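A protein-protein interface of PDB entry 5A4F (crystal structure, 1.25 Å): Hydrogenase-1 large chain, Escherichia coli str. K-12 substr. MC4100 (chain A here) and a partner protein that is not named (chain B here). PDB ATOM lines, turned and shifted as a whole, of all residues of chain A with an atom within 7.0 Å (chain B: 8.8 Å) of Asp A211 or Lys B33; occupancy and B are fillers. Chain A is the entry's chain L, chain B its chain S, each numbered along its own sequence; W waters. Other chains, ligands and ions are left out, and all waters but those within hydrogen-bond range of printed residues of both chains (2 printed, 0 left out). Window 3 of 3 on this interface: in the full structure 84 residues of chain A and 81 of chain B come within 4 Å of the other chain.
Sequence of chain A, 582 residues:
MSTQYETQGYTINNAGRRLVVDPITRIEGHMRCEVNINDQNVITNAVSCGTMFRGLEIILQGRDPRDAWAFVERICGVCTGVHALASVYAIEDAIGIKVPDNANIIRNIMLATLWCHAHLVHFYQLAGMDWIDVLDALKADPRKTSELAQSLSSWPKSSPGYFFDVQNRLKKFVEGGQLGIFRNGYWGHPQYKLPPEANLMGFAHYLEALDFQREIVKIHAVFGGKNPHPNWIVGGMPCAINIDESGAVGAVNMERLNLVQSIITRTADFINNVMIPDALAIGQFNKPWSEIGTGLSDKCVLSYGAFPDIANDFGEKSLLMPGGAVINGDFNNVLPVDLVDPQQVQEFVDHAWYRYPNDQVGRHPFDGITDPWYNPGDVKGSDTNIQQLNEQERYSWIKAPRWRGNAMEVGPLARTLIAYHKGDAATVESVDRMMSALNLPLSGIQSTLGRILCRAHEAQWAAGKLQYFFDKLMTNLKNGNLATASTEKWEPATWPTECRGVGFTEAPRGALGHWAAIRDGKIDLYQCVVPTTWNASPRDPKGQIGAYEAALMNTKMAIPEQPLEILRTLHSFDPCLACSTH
NH2 of Arg A169 is in salt-bridge range of OD1 of Asp B34 (2.8 Å). The guanidinium group (NH2) of Arg A169 lies within hydrogen-bond range of the side-chain hydroxyl (OG) of Ser B38, at 3.0 Å. The side-chain carboxylate (OD2) of Asp A211 is in salt-bridge range of the side-chain amino group (NZ) of Lys B33, 2.7 Å away. The side-chain amide nitrogen of Gln A213 is in hydrogen-bond range of the backbone carbonyl oxygen of Ile B25 (2.9 Å). OE1 of Gln A213 lies within hydrogen-bond range of NH1 of Arg B26.
The backbone carbonyl oxygen (O) of Leu A210 is in hydrogen-bond range of the side-chain amide nitrogen (NE2) of Gln A213 (2.8 Å). NE of Arg A214 is in salt-bridge range of OE2 of Glu A215, 3.6 Å away. OG of Ser B27 is in hydrogen-bond range of O of Pro B30 (2.6 Å). N of Leu B39 sits at hydrogen-bond distance from O of Asp B34 (3.4 Å).
Among the printed residues, pairs that only touch across the chains: Arg A169 with Leu B37 (3.6 Å), Leu A210 with Lys B33 (3.9 Å), Asp A211 with Leu B31 (3.6 Å), Arg A214 with Arg B26 (3.6 Å), Arg A214 with Ser B27 (3.6 Å), Arg A214 with Ala B28 (3.8 Å) and Arg A214 with Leu B31 (3.6 Å).
Printed residues of chain B within 4 Å of Arg A169: Asp B34, Leu B37 and Ser B38. Of the printed residues of chain B, Leu A210 touches Lys B33 (3.9 Å). Asp A211 touches just these residues of chain B: Leu B31 and Lys B33. Printed residues of chain B within 4 Å of Gln A213: Ile B25 (2.9 Å) and Arg B26 (3.2 Å). Of the printed residues of chain B, Arg A214 touches Arg B26, Ser B27, Ala B28 and Leu B31. Printed residues of chain A within 4 Å of Leu B37: Arg A169. The nearest residue of chain A that does not touch Lys B33 is Leu A207 (4.1 Å). The nearest printed residue of chain A that does not touch Ala B28 is Glu A215 (6.0 Å).
Of the 19 printed residues of chain B, 9 touch a printed residue of chain A. Among the printed residues, Asp or Glu carboxylates within 4 Å of a Lys or Arg side-chain nitrogen of the other chain: Arg A169 with Asp B34 (2.8 Å) and Asp A211 with Lys B33 (2.7 Å).
Water W2 lies within hydrogen-bond range of the side-chain hydroxyl of Tyr A206 (2.6 Å), the backbone carbonyl oxygen of Gln A125 (2.8 Å) and the backbone carbonyl oxygen of Leu B48 (2.8 Å). Water W1 lies within hydrogen-bond range of the side-chain carboxylate (OD1) of Asp A211 (2.8 Å), the backbone NH (N) of Lys B33 (2.9 Å) and the backbone NH (N) of Ala B32 (3.3 Å).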
ATOM      1  N   GLN A 125     -17.863  20.452   2.726  1.00  0.00           N
ATOM      2  CA  GLN A 125     -16.920  20.351   1.625  1.00  0.00           C
ATOM      3  C   GLN A 125     -15.808  19.327   1.838  1.00  0.00           C
ATOM      4  O   GLN A 125     -15.329  18.762   0.844  1.00  0.00           O
ATOM      5  CB  GLN A 125     -16.293  21.712   1.267  1.00  0.00           C
ATOM      6  CG  GLN A 125     -17.160  22.572   0.341  1.00  0.00           C
ATOM      7  CD  GLN A 125     -18.507  22.917   0.971  1.00  0.00           C
ATOM      8  OE1 GLN A 125     -18.558  23.563   2.029  1.00  0.00           O
ATOM      9  NE2 GLN A 125     -19.611  22.466   0.350  1.00  0.00           N
ATOM     10  N   LYS A 157     -35.922  26.008   2.874  1.00  0.00           N
ATOM     11  CA  LYS A 157     -35.636  25.550   1.542  1.00  0.00           C
ATOM     12  C   LYS A 157     -35.763  24.042   1.432  1.00  0.00           C
ATOM     13  O   LYS A 157     -34.799  23.304   1.595  1.00  0.00           O
ATOM     14  CB  LYS A 157     -34.271  25.994   1.096  1.00  0.00           C
ATOM     15  CG  LYS A 157     -34.100  27.481   1.006  1.00  0.00           C
ATOM     16  CD  LYS A 157     -32.728  27.823   0.347  1.00  0.00           C
ATOM     17  CE  LYS A 157     -32.516  29.299   0.270  1.00  0.00           C
ATOM     18  NZ  LYS A 157     -31.224  29.483  -0.432  1.00  0.00           N
ATOM     19  N   ARG A 169     -29.880  19.429 -11.886  1.00  0.00           N
ATOM     20  CA  ARG A 169     -28.574  20.087 -12.099  1.00  0.00           C
ATOM     21  C   ARG A 169     -27.427  19.075 -11.974  1.00  0.00           C
ATOM     22  O   ARG A 169     -26.514  19.078 -12.777  1.00  0.00           O
ATOM     23  CB  ARG A 169     -28.366  21.172 -11.081  1.00  0.00           C
ATOM     24  CG  ARG A 169     -27.103  21.998 -11.287  1.00  0.00           C
ATOM     25  CD  ARG A 169     -27.475  23.417 -11.615  1.00  0.00           C
ATOM     26  NE  ARG A 169     -26.306  24.222 -11.958  1.00  0.00           N
ATOM     27  CZ  ARG A 169     -25.854  25.270 -11.264  1.00  0.00           C
ATOM     28  NH1 ARG A 169     -26.415  25.699 -10.116  1.00  0.00           N
ATOM     29  NH2 ARG A 169     -24.809  25.924 -11.749  1.00  0.00           N
ATOM     30  N   HIS A 205     -27.653  20.554   0.604  1.00  0.00           N
ATOM     31  CA  HIS A 205     -27.049  21.327   1.675  1.00  0.00           C
ATOM     32  C   HIS A 205     -25.583  21.592   1.464  1.00  0.00           C
ATOM     33  O   HIS A 205     -25.100  22.657   1.818  1.00  0.00           O
ATOM     34  CB  HIS A 205     -27.335  20.685   3.029  1.00  0.00           C
ATOM     35  CG  HIS A 205     -28.800  20.703   3.353  1.00  0.00           C
ATOM     36  ND1 HIS A 205     -29.318  19.993   4.409  1.00  0.00           N
ATOM     37  CD2 HIS A 205     -29.857  21.307   2.751  1.00  0.00           C
ATOM     38  CE1 HIS A 205     -30.628  20.163   4.454  1.00  0.00           C
ATOM     39  NE2 HIS A 205     -30.978  20.984   3.485  1.00  0.00           N
ATOM     40  N   TYR A 206     -24.882  20.646   0.870  1.00  0.00           N
ATOM     41  CA  TYR A 206     -23.478  20.866   0.464  1.00  0.00           C
ATOM     42  C   TYR A 206     -23.407  22.122  -0.395  1.00  0.00           C
ATOM     43  O   TYR A 206     -22.540  22.979  -0.163  1.00  0.00           O
ATOM     44  CB  TYR A 206     -22.951  19.618  -0.265  1.00  0.00           C
ATOM     45  CG  TYR A 206     -21.618  19.731  -0.954  1.00  0.00           C
ATOM     46  CD1 TYR A 206     -21.481  20.400  -2.145  1.00  0.00           C
ATOM     47  CD2 TYR A 206     -20.504  19.076  -0.464  1.00  0.00           C
ATOM     48  CE1 TYR A 206     -20.234  20.564  -2.764  1.00  0.00           C
ATOM     49  CE2 TYR A 206     -19.284  19.154  -1.093  1.00  0.00           C
ATOM     50  CZ  TYR A 206     -19.146  19.885  -2.242  1.00  0.00           C
ATOM     51  OH  TYR A 206     -17.942  20.034  -2.885  1.00  0.00           O
ATOM     52  N   LEU A 207     -24.282  22.215  -1.372  1.00  0.00           N
ATOM     53  CA  LEU A 207     -24.285  23.379  -2.253  1.00  0.00           C
ATOM     54  C   LEU A 207     -24.692  24.658  -1.551  1.00  0.00           C
ATOM     55  O   LEU A 207     -24.095  25.719  -1.728  1.00  0.00           O
ATOM     56  CB  LEU A 207     -25.195  23.135  -3.448  1.00  0.00           C
ATOM     57  CG  LEU A 207     -24.769  21.978  -4.379  1.00  0.00           C
ATOM     58  CD1 LEU A 207     -25.815  21.838  -5.465  1.00  0.00           C
ATOM     59  CD2 LEU A 207     -23.460  22.187  -5.064  1.00  0.00           C
ATOM     60  N   GLU A 208     -25.682  24.586  -0.691  1.00  0.00           N
ATOM     61  CA  GLU A 208     -26.080  25.759   0.096  1.00  0.00           C
ATOM     62  C   GLU A 208     -24.958  26.224   0.998  1.00  0.00           C
ATOM     63  O   GLU A 208     -24.760  27.448   1.150  1.00  0.00           O
ATOM     64  CB  GLU A 208     -27.322  25.459   0.946  1.00  0.00           C
ATOM     65  CG  GLU A 208     -28.627  25.226   0.164  1.00  0.00           C
ATOM     66  CD  GLU A 208     -29.845  25.086   1.052  1.00  0.00           C
ATOM     67  OE1 GLU A 208     -29.992  25.882   2.003  1.00  0.00           O
ATOM     68  OE2 GLU A 208     -30.660  24.154   0.790  1.00  0.00           O
ATOM     69  N   ALA A 209     -24.225  25.312   1.605  1.00  0.00           N
ATOM     70  CA  ALA A 209     -23.113  25.682   2.478  1.00  0.00           C
ATOM     71  C   ALA A 209     -21.959  26.250   1.691  1.00  0.00           C
ATOM     72  O   ALA A 209     -21.348  27.208   2.160  1.00  0.00           O
ATOM     73  CB  ALA A 209     -22.631  24.484   3.246  1.00  0.00           C
ATOM     74  N   LEU A 210     -21.672  25.706   0.528  1.00  0.00           N
ATOM     75  CA  LEU A 210     -20.629  26.288  -0.344  1.00  0.00           C
ATOM     76  C   LEU A 210     -20.965  27.731  -0.674  1.00  0.00           C
ATOM     77  O   LEU A 210     -20.073  28.607  -0.654  1.00  0.00           O
ATOM     78  CB  LEU A 210     -20.503  25.452  -1.623  1.00  0.00           C
ATOM     79  CG  LEU A 210     -19.409  25.876  -2.596  1.00  0.00           C
ATOM     80  CD1 LEU A 210     -18.023  25.964  -1.981  1.00  0.00           C
ATOM     81  CD2 LEU A 210     -19.425  24.923  -3.797  1.00  0.00           C
ATOM     82  N   ASP A 211     -22.234  28.034  -0.956  1.00  0.00           N
ATOM     83  CA  ASP A 211     -22.598  29.424  -1.179  1.00  0.00           C
ATOM     84  C   ASP A 211     -22.523  30.274   0.097  1.00  0.00           C
ATOM     85  O   ASP A 211     -21.966  31.371   0.098  1.00  0.00           O
ATOM     86  CB  ASP A 211     -24.007  29.536  -1.740  1.00  0.00           C
ATOM     87  CG  ASP A 211     -24.171  29.001  -3.148  1.00  0.00           C
ATOM     88  OD1 ASP A 211     -23.199  28.777  -3.852  1.00  0.00           O
ATOM     89  OD2 ASP A 211     -25.383  28.918  -3.561  1.00  0.00           O
ATOM     90  N   PHE A 212     -23.110  29.779   1.188  1.00  0.00           N
ATOM     91  CA  PHE A 212     -23.289  30.575   2.376  1.00  0.00           C
ATOM     92  C   PHE A 212     -21.981  30.901   3.099  1.00  0.00           C
ATOM     93  O   PHE A 212     -21.868  31.968   3.704  1.00  0.00           O
ATOM     94  CB  PHE A 212     -24.272  29.934   3.345  1.00  0.00           C
ATOM     95  CG  PHE A 212     -24.492  30.777   4.558  1.00  0.00           C
ATOM     96  CD1 PHE A 212     -25.182  31.985   4.461  1.00  0.00           C
ATOM     97  CD2 PHE A 212     -23.904  30.475   5.762  1.00  0.00           C
ATOM     98  CE1 PHE A 212     -25.272  32.838   5.537  1.00  0.00           C
ATOM     99  CE2 PHE A 212     -23.998  31.331   6.846  1.00  0.00           C
ATOM    100  CZ  PHE A 212     -24.664  32.516   6.715  1.00  0.00           C
ATOM    101  N   GLN A 213     -21.008  29.987   3.078  1.00  0.00           N
ATOM    102  CA  GLN A 213     -19.840  30.200   3.854  1.00  0.00           C
ATOM    103  C   GLN A 213     -19.132  31.543   3.539  1.00  0.00           C
ATOM    104  O   GLN A 213     -18.482  32.129   4.400  1.00  0.00           O
ATOM    105  CB  GLN A 213     -18.841  29.032   3.768  1.00  0.00           C
ATOM    106  CG  GLN A 213     -18.387  28.620   2.352  1.00  0.00           C
ATOM    107  CD  GLN A 213     -17.463  29.589   1.661  1.00  0.00           C
ATOM    108  OE1 GLN A 213     -16.544  30.168   2.271  1.00  0.00           O
ATOM    109  NE2 GLN A 213     -17.673  29.736   0.386  1.00  0.00           N
ATOM    110  N   ARG A 214     -19.275  32.028   2.302  1.00  0.00           N
ATOM    111  CA  ARG A 214     -18.630  33.256   1.886  1.00  0.00           C
ATOM    112  C   ARG A 214     -19.136  34.434   2.721  1.00  0.00           C
ATOM    113  O   ARG A 214     -18.415  35.408   2.869  1.00  0.00           O
ATOM    114  CB  ARG A 214     -18.845  33.510   0.388  1.00  0.00           C
ATOM    115  CG  ARG A 214     -20.178  34.108   0.048  1.00  0.00           C
ATOM    116  CD  ARG A 214     -20.404  34.097  -1.458  1.00  0.00           C
ATOM    117  NE  ARG A 214     -21.550  34.938  -1.856  1.00  0.00           N
ATOM    118  CZ  ARG A 214     -22.814  34.625  -1.719  1.00  0.00           C
ATOM    119  NH1 ARG A 214     -23.187  33.448  -1.251  1.00  0.00           N
ATOM    120  NH2 ARG A 214     -23.735  35.510  -2.087  1.00  0.00           N
ATOM    121  N   GLU A 215     -20.372  34.362   3.204  1.00  0.00           N
ATOM    122  CA  GLU A 215     -20.940  35.469   3.936  1.00  0.00           C
ATOM    123  C   GLU A 215     -20.353  35.591   5.342  1.00  0.00           C
ATOM    124  O   GLU A 215     -20.195  36.710   5.853  1.00  0.00           O
ATOM    125  CB  GLU A 215     -22.444  35.277   4.021  1.00  0.00           C
ATOM    126  CG  GLU A 215     -23.171  35.288   2.678  1.00  0.00           C
ATOM    127  CD  GLU A 215     -23.057  36.667   2.059  1.00  0.00           C
ATOM    128  OE1 GLU A 215     -23.575  37.663   2.538  1.00  0.00           O
ATOM    129  OE2 GLU A 215     -22.243  36.868   1.151  1.00  0.00           O
ATOM    130  N   ILE A 216     -20.038  34.466   5.969  1.00  0.00           N
ATOM    131  CA  ILE A 216     -19.633  34.450   7.367  1.00  0.00           C
ATOM    132  C   ILE A 216     -18.401  35.335   7.562  1.00  0.00           C
ATOM    133  O   ILE A 216     -18.290  36.096   8.523  1.00  0.00           O
ATOM    134  CB  ILE A 216     -19.322  33.015   7.824  1.00  0.00           C
ATOM    135  CG1 ILE A 216     -20.551  32.106   7.704  1.00  0.00           C
ATOM    136  CG2 ILE A 216     -18.793  33.008   9.250  1.00  0.00           C
ATOM    137  CD1 ILE A 216     -20.296  30.626   7.975  1.00  0.00           C
ATOM    138  N   PHE A 270     -28.198  29.492   9.748  1.00  0.00           N
ATOM    139  CA  PHE A 270     -27.750  28.419   8.850  1.00  0.00           C
ATOM    140  C   PHE A 270     -27.215  27.205   9.661  1.00  0.00           C
ATOM    141  O   PHE A 270     -27.533  26.023   9.395  1.00  0.00           O
ATOM    142  CB  PHE A 270     -26.677  28.946   7.881  1.00  0.00           C
ATOM    143  CG  PHE A 270     -26.426  28.009   6.713  1.00  0.00           C
ATOM    144  CD1 PHE A 270     -25.583  26.940   6.804  1.00  0.00           C
ATOM    145  CD2 PHE A 270     -27.097  28.214   5.524  1.00  0.00           C
ATOM    146  CE1 PHE A 270     -25.409  26.055   5.757  1.00  0.00           C
ATOM    147  CE2 PHE A 270     -26.877  27.372   4.462  1.00  0.00           C
ATOM    148  CZ  PHE A 270     -26.095  26.260   4.597  1.00  0.00           C
ATOM    149  N   ARG B   6     -17.318  21.495 -20.902  1.00  0.00           N
ATOM    150  CA  ARG B   6     -16.643  22.569 -20.141  1.00  0.00           C
ATOM    151  C   ARG B   6     -15.150  22.372 -20.217  1.00  0.00           C
ATOM    152  O   ARG B   6     -14.679  21.269 -20.340  1.00  0.00           O
ATOM    153  CB  ARG B   6     -17.194  22.584 -18.727  1.00  0.00           C
ATOM    154  CG  ARG B   6     -18.636  23.109 -18.666  1.00  0.00           C
ATOM    155  CD  ARG B   6     -19.311  22.783 -17.363  1.00  0.00           C
ATOM    156  NE  ARG B   6     -19.771  21.380 -17.250  1.00  0.00           N
ATOM    157  CZ  ARG B   6     -19.321  20.495 -16.381  1.00  0.00           C
ATOM    158  NH1 ARG B   6     -18.388  20.804 -15.494  1.00  0.00           N
ATOM    159  NH2 ARG B   6     -19.850  19.261 -16.359  1.00  0.00           N
ATOM    160  N   PHE B  24     -10.817  31.604  -3.632  1.00  0.00           N
ATOM    161  CA  PHE B  24     -11.647  31.235  -4.751  1.00  0.00           C
ATOM    162  C   PHE B  24     -13.052  30.904  -4.315  1.00  0.00           C
ATOM    163  O   PHE B  24     -14.040  31.365  -4.908  1.00  0.00           O
ATOM    164  CB  PHE B  24     -11.009  30.090  -5.518  1.00  0.00           C
ATOM    165  CG  PHE B  24     -11.898  29.419  -6.513  1.00  0.00           C
ATOM    166  CD1 PHE B  24     -12.361  30.094  -7.601  1.00  0.00           C
ATOM    167  CD2 PHE B  24     -12.300  28.119  -6.315  1.00  0.00           C
ATOM    168  CE1 PHE B  24     -13.222  29.453  -8.489  1.00  0.00           C
ATOM    169  CE2 PHE B  24     -13.124  27.452  -7.206  1.00  0.00           C
ATOM    170  CZ  PHE B  24     -13.576  28.126  -8.290  1.00  0.00           C
ATOM    171  N   ILE B  25     -13.170  30.113  -3.240  1.00  0.00           N
ATOM    172  CA  ILE B  25     -14.530  29.722  -2.804  1.00  0.00           C
ATOM    173  C   ILE B  25     -15.317  30.864  -2.173  1.00  0.00           C
ATOM    174  O   ILE B  25     -16.541  30.721  -2.049  1.00  0.00           O
ATOM    175  CB  ILE B  25     -14.626  28.424  -1.962  1.00  0.00           C
ATOM    176  CG1 ILE B  25     -14.051  28.597  -0.581  1.00  0.00           C
ATOM    177  CG2 ILE B  25     -13.998  27.261  -2.699  1.00  0.00           C
ATOM    178  CD1 ILE B  25     -14.355  27.428   0.361  1.00  0.00           C
ATOM    179  N   ARG B  26     -14.668  31.991  -1.869  1.00  0.00           N
ATOM    180  CA  ARG B  26     -15.381  33.156  -1.399  1.00  0.00           C
ATOM    181  C   ARG B  26     -16.041  33.931  -2.531  1.00  0.00           C
ATOM    182  O   ARG B  26     -16.810  34.851  -2.258  1.00  0.00           O
ATOM    183  CB  ARG B  26     -14.478  34.161  -0.649  1.00  0.00           C
ATOM    184  CG  ARG B  26     -13.684  33.659   0.531  1.00  0.00           C
ATOM    185  CD  ARG B  26     -14.523  33.161   1.632  1.00  0.00           C
ATOM    186  NE  ARG B  26     -13.622  32.826   2.749  1.00  0.00           N
ATOM    187  CZ  ARG B  26     -13.015  31.670   2.936  1.00  0.00           C
ATOM    188  NH1 ARG B  26     -13.412  30.584   2.308  1.00  0.00           N
ATOM    189  NH2 ARG B  26     -12.080  31.608   3.833  1.00  0.00           N
ATOM    190  N   SER B  27     -15.784  33.580  -3.796  1.00  0.00           N
ATOM    191  CA  SER B  27     -16.338  34.385  -4.889  1.00  0.00           C
ATOM    192  C   SER B  27     -17.834  34.641  -4.762  1.00  0.00           C
ATOM    193  O   SER B  27     -18.629  33.728  -4.546  1.00  0.00           O
ATOM    194  CB  SER B  27     -16.064  33.682  -6.214  1.00  0.00           C
ATOM    195  OG  SER B  27     -16.486  34.517  -7.303  1.00  0.00           O
ATOM    196  N   ALA B  28     -18.220  35.893  -4.975  1.00  0.00           N
ATOM    197  CA  ALA B  28     -19.612  36.294  -4.862  1.00  0.00           C
ATOM    198  C   ALA B  28     -20.322  36.260  -6.212  1.00  0.00           C
ATOM    199  O   ALA B  28     -21.533  36.137  -6.265  1.00  0.00           O
ATOM    200  CB  ALA B  28     -19.704  37.657  -4.274  1.00  0.00           C
ATOM    201  N   HIS B  29     -19.602  36.453  -7.296  1.00  0.00           N
ATOM    202  CA  HIS B  29     -20.213  36.581  -8.621  1.00  0.00           C
ATOM    203  C   HIS B  29     -19.189  36.350  -9.702  1.00  0.00           C
ATOM    204  O   HIS B  29     -18.373  37.228  -9.934  1.00  0.00           O
ATOM    205  CB  HIS B  29     -20.944  37.965  -8.798  1.00  0.00           C
ATOM    206  CG  HIS B  29     -20.203  39.177  -8.318  1.00  0.00           C
ATOM    207  ND1 HIS B  29     -20.538  39.804  -7.134  1.00  0.00           N
ATOM    208  CD2 HIS B  29     -19.159  39.871  -8.839  1.00  0.00           C
ATOM    209  CE1 HIS B  29     -19.754  40.848  -6.977  1.00  0.00           C
ATOM    210  NE2 HIS B  29     -18.889  40.890  -7.973  1.00  0.00           N
ATOM    211  N   PRO B  30     -19.225  35.205 -10.349  1.00  0.00           N
ATOM    212  CA  PRO B  30     -20.084  34.062 -10.104  1.00  0.00           C
ATOM    213  C   PRO B  30     -19.722  33.363  -8.812  1.00  0.00           C
ATOM    214  O   PRO B  30     -18.552  33.346  -8.412  1.00  0.00           O
ATOM    215  CB  PRO B  30     -19.738  33.123 -11.280  1.00  0.00           C
ATOM    216  CG  PRO B  30     -18.337  33.501 -11.648  1.00  0.00           C
ATOM    217  CD  PRO B  30     -18.250  34.961 -11.444  1.00  0.00           C
ATOM    218  N   LEU B  31     -20.705  32.720  -8.179  1.00  0.00           N
ATOM    219  CA  LEU B  31     -20.413  31.840  -7.072  1.00  0.00           C
ATOM    220  C   LEU B  31     -19.456  30.733  -7.496  1.00  0.00           C
ATOM    221  O   LEU B  31     -19.566  30.229  -8.624  1.00  0.00           O
ATOM    222  CB  LEU B  31     -21.730  31.222  -6.553  1.00  0.00           C
ATOM    223  CG  LEU B  31     -22.771  32.211  -6.007  1.00  0.00           C
ATOM    224  CD1 LEU B  31     -24.157  31.557  -5.923  1.00  0.00           C
ATOM    225  CD2 LEU B  31     -22.264  32.747  -4.687  1.00  0.00           C
ATOM    226  N   ALA B  32     -18.581  30.295  -6.612  1.00  0.00           N
ATOM    227  CA  ALA B  32     -17.716  29.176  -6.914  1.00  0.00           C
ATOM    228  C   ALA B  32     -18.490  27.934  -7.321  1.00  0.00           C
ATOM    229  O   ALA B  32     -18.072  27.217  -8.237  1.00  0.00           O
ATOM    230  CB  ALA B  32     -16.776  28.899  -5.746  1.00  0.00           C
ATOM    231  N   LYS B  33     -19.633  27.707  -6.701  1.00  0.00           N
ATOM    232  CA  LYS B  33     -20.536  26.663  -7.076  1.00  0.00           C
ATOM    233  C   LYS B  33     -20.831  26.699  -8.565  1.00  0.00           C
ATOM    234  O   LYS B  33     -20.849  25.657  -9.242  1.00  0.00           O
ATOM    235  CB  LYS B  33     -21.832  26.831  -6.309  1.00  0.00           C
ATOM    236  CG  LYS B  33     -22.929  25.863  -6.680  1.00  0.00           C
ATOM    237  CD  LYS B  33     -24.302  26.189  -6.047  1.00  0.00           C
ATOM    238  CE  LYS B  33     -24.969  27.410  -6.672  1.00  0.00           C
ATOM    239  NZ  LYS B  33     -26.179  27.797  -5.929  1.00  0.00           N
ATOM    240  N   ASP B  34     -21.199  27.873  -9.075  1.00  0.00           N
ATOM    241  CA  ASP B  34     -21.572  27.979 -10.500  1.00  0.00           C
ATOM    242  C   ASP B  34     -20.357  27.907 -11.422  1.00  0.00           C
ATOM    243  O   ASP B  34     -20.449  27.406 -12.529  1.00  0.00           O
ATOM    244  CB  ASP B  34     -22.376  29.269 -10.682  1.00  0.00           C
ATOM    245  CG  ASP B  34     -23.749  29.188 -10.059  1.00  0.00           C
ATOM    246  OD1 ASP B  34     -24.390  28.131 -10.162  1.00  0.00           O
ATOM    247  OD2 ASP B  34     -24.237  30.191  -9.494  1.00  0.00           O
ATOM    248  N   VAL B  35     -19.183  28.359 -10.954  1.00  0.00           N
ATOM    249  CA  VAL B  35     -17.963  28.139 -11.717  1.00  0.00           C
ATOM    250  C   VAL B  35     -17.740  26.634 -11.937  1.00  0.00           C
ATOM    251  O   VAL B  35     -17.516  26.220 -13.094  1.00  0.00           O
ATOM    252  CB  VAL B  35     -16.749  28.788 -11.036  1.00  0.00           C
ATOM    253  CG1 VAL B  35     -15.473  28.422 -11.768  1.00  0.00           C
ATOM    254  CG2 VAL B  35     -16.892  30.292 -10.918  1.00  0.00           C
ATOM    255  N   ILE B  36     -17.832  25.886 -10.850  1.00  0.00           N
ATOM    256  CA  ILE B  36     -17.560  24.452 -10.864  1.00  0.00           C
ATOM    257  C   ILE B  36     -18.627  23.683 -11.646  1.00  0.00           C
ATOM    258  O   ILE B  36     -18.355  22.750 -12.425  1.00  0.00           O
ATOM    259  CB  ILE B  36     -17.443  23.926  -9.407  1.00  0.00           C
ATOM    260  CG1 ILE B  36     -16.132  24.529  -8.827  1.00  0.00           C
ATOM    261  CG2 ILE B  36     -17.457  22.390  -9.356  1.00  0.00           C
ATOM    262  CD1 ILE B  36     -16.034  24.379  -7.317  1.00  0.00           C
ATOM    263  N   LEU B  37     -19.890  24.052 -11.462  1.00  0.00           N
ATOM    264  CA  LEU B  37     -20.958  23.326 -12.109  1.00  0.00           C
ATOM    265  C   LEU B  37     -21.128  23.681 -13.568  1.00  0.00           C
ATOM    266  O   LEU B  37     -21.519  22.786 -14.383  1.00  0.00           O
ATOM    267  CB  LEU B  37     -22.268  23.467 -11.333  1.00  0.00           C
ATOM    268  CG  LEU B  37     -22.266  22.765  -9.942  1.00  0.00           C
ATOM    269  CD1 LEU B  37     -23.551  23.067  -9.223  1.00  0.00           C
ATOM    270  CD2 LEU B  37     -22.079  21.225  -9.952  1.00  0.00           C
ATOM    271  N   SER B  38     -20.926  24.945 -13.923  1.00  0.00           N
ATOM    272  CA  SER B  38     -21.314  25.478 -15.230  1.00  0.00           C
ATOM    273  C   SER B  38     -20.267  26.054 -16.135  1.00  0.00           C
ATOM    274  O   SER B  38     -20.445  26.094 -17.369  1.00  0.00           O
ATOM    275  CB  SER B  38     -22.479  26.493 -15.041  1.00  0.00           C
ATOM    276  OG  SER B  38     -23.590  25.822 -14.513  1.00  0.00           O
ATOM    277  N   LEU B  39     -19.167  26.511 -15.582  1.00  0.00           N
ATOM    278  CA  LEU B  39     -18.195  27.246 -16.401  1.00  0.00           C
ATOM    279  C   LEU B  39     -16.956  26.446 -16.772  1.00  0.00           C
ATOM    280  O   LEU B  39     -16.405  26.661 -17.866  1.00  0.00           O
ATOM    281  CB  LEU B  39     -17.767  28.527 -15.687  1.00  0.00           C
ATOM    282  CG  LEU B  39     -18.915  29.529 -15.450  1.00  0.00           C
ATOM    283  CD1 LEU B  39     -18.335  30.795 -14.877  1.00  0.00           C
ATOM    284  CD2 LEU B  39     -19.746  29.831 -16.696  1.00  0.00           C
ATOM    285  N   ILE B  40     -16.470  25.619 -15.874  1.00  0.00           N
ATOM    286  CA  ILE B  40     -15.249  24.827 -16.078  1.00  0.00           C
ATOM    287  C   ILE B  40     -15.548  23.402 -15.675  1.00  0.00           C
ATOM    288  O   ILE B  40     -16.591  23.158 -15.058  1.00  0.00           O
ATOM    289  CB  ILE B  40     -14.032  25.349 -15.267  1.00  0.00           C
ATOM    290  CG1 ILE B  40     -14.256  25.193 -13.741  1.00  0.00           C
ATOM    291  CG2 ILE B  40     -13.709  26.768 -15.687  1.00  0.00           C
ATOM    292  CD1 ILE B  40     -13.075  25.532 -12.863  1.00  0.00           C
ATOM    293  N   LEU B  48     -10.743  19.350  -2.740  1.00  0.00           N
ATOM    294  CA  LEU B  48     -12.183  19.188  -2.868  1.00  0.00           C
ATOM    295  C   LEU B  48     -12.636  17.835  -3.419  1.00  0.00           C
ATOM    296  O   LEU B  48     -13.803  17.484  -3.306  1.00  0.00           O
ATOM    297  CB  LEU B  48     -12.758  20.284  -3.785  1.00  0.00           C
ATOM    298  CG  LEU B  48     -12.592  21.742  -3.290  1.00  0.00           C
ATOM    299  CD1 LEU B  48     -13.044  22.732  -4.357  1.00  0.00           C
ATOM    300  CD2 LEU B  48     -13.349  21.939  -1.982  1.00  0.00           C
HETATM  301  O   HOH W   1     -20.379  28.995  -4.167  1.00  0.00           O
HETATM  302  O   HOH W   2     -15.777  18.897  -1.874  1.00  0.00           O
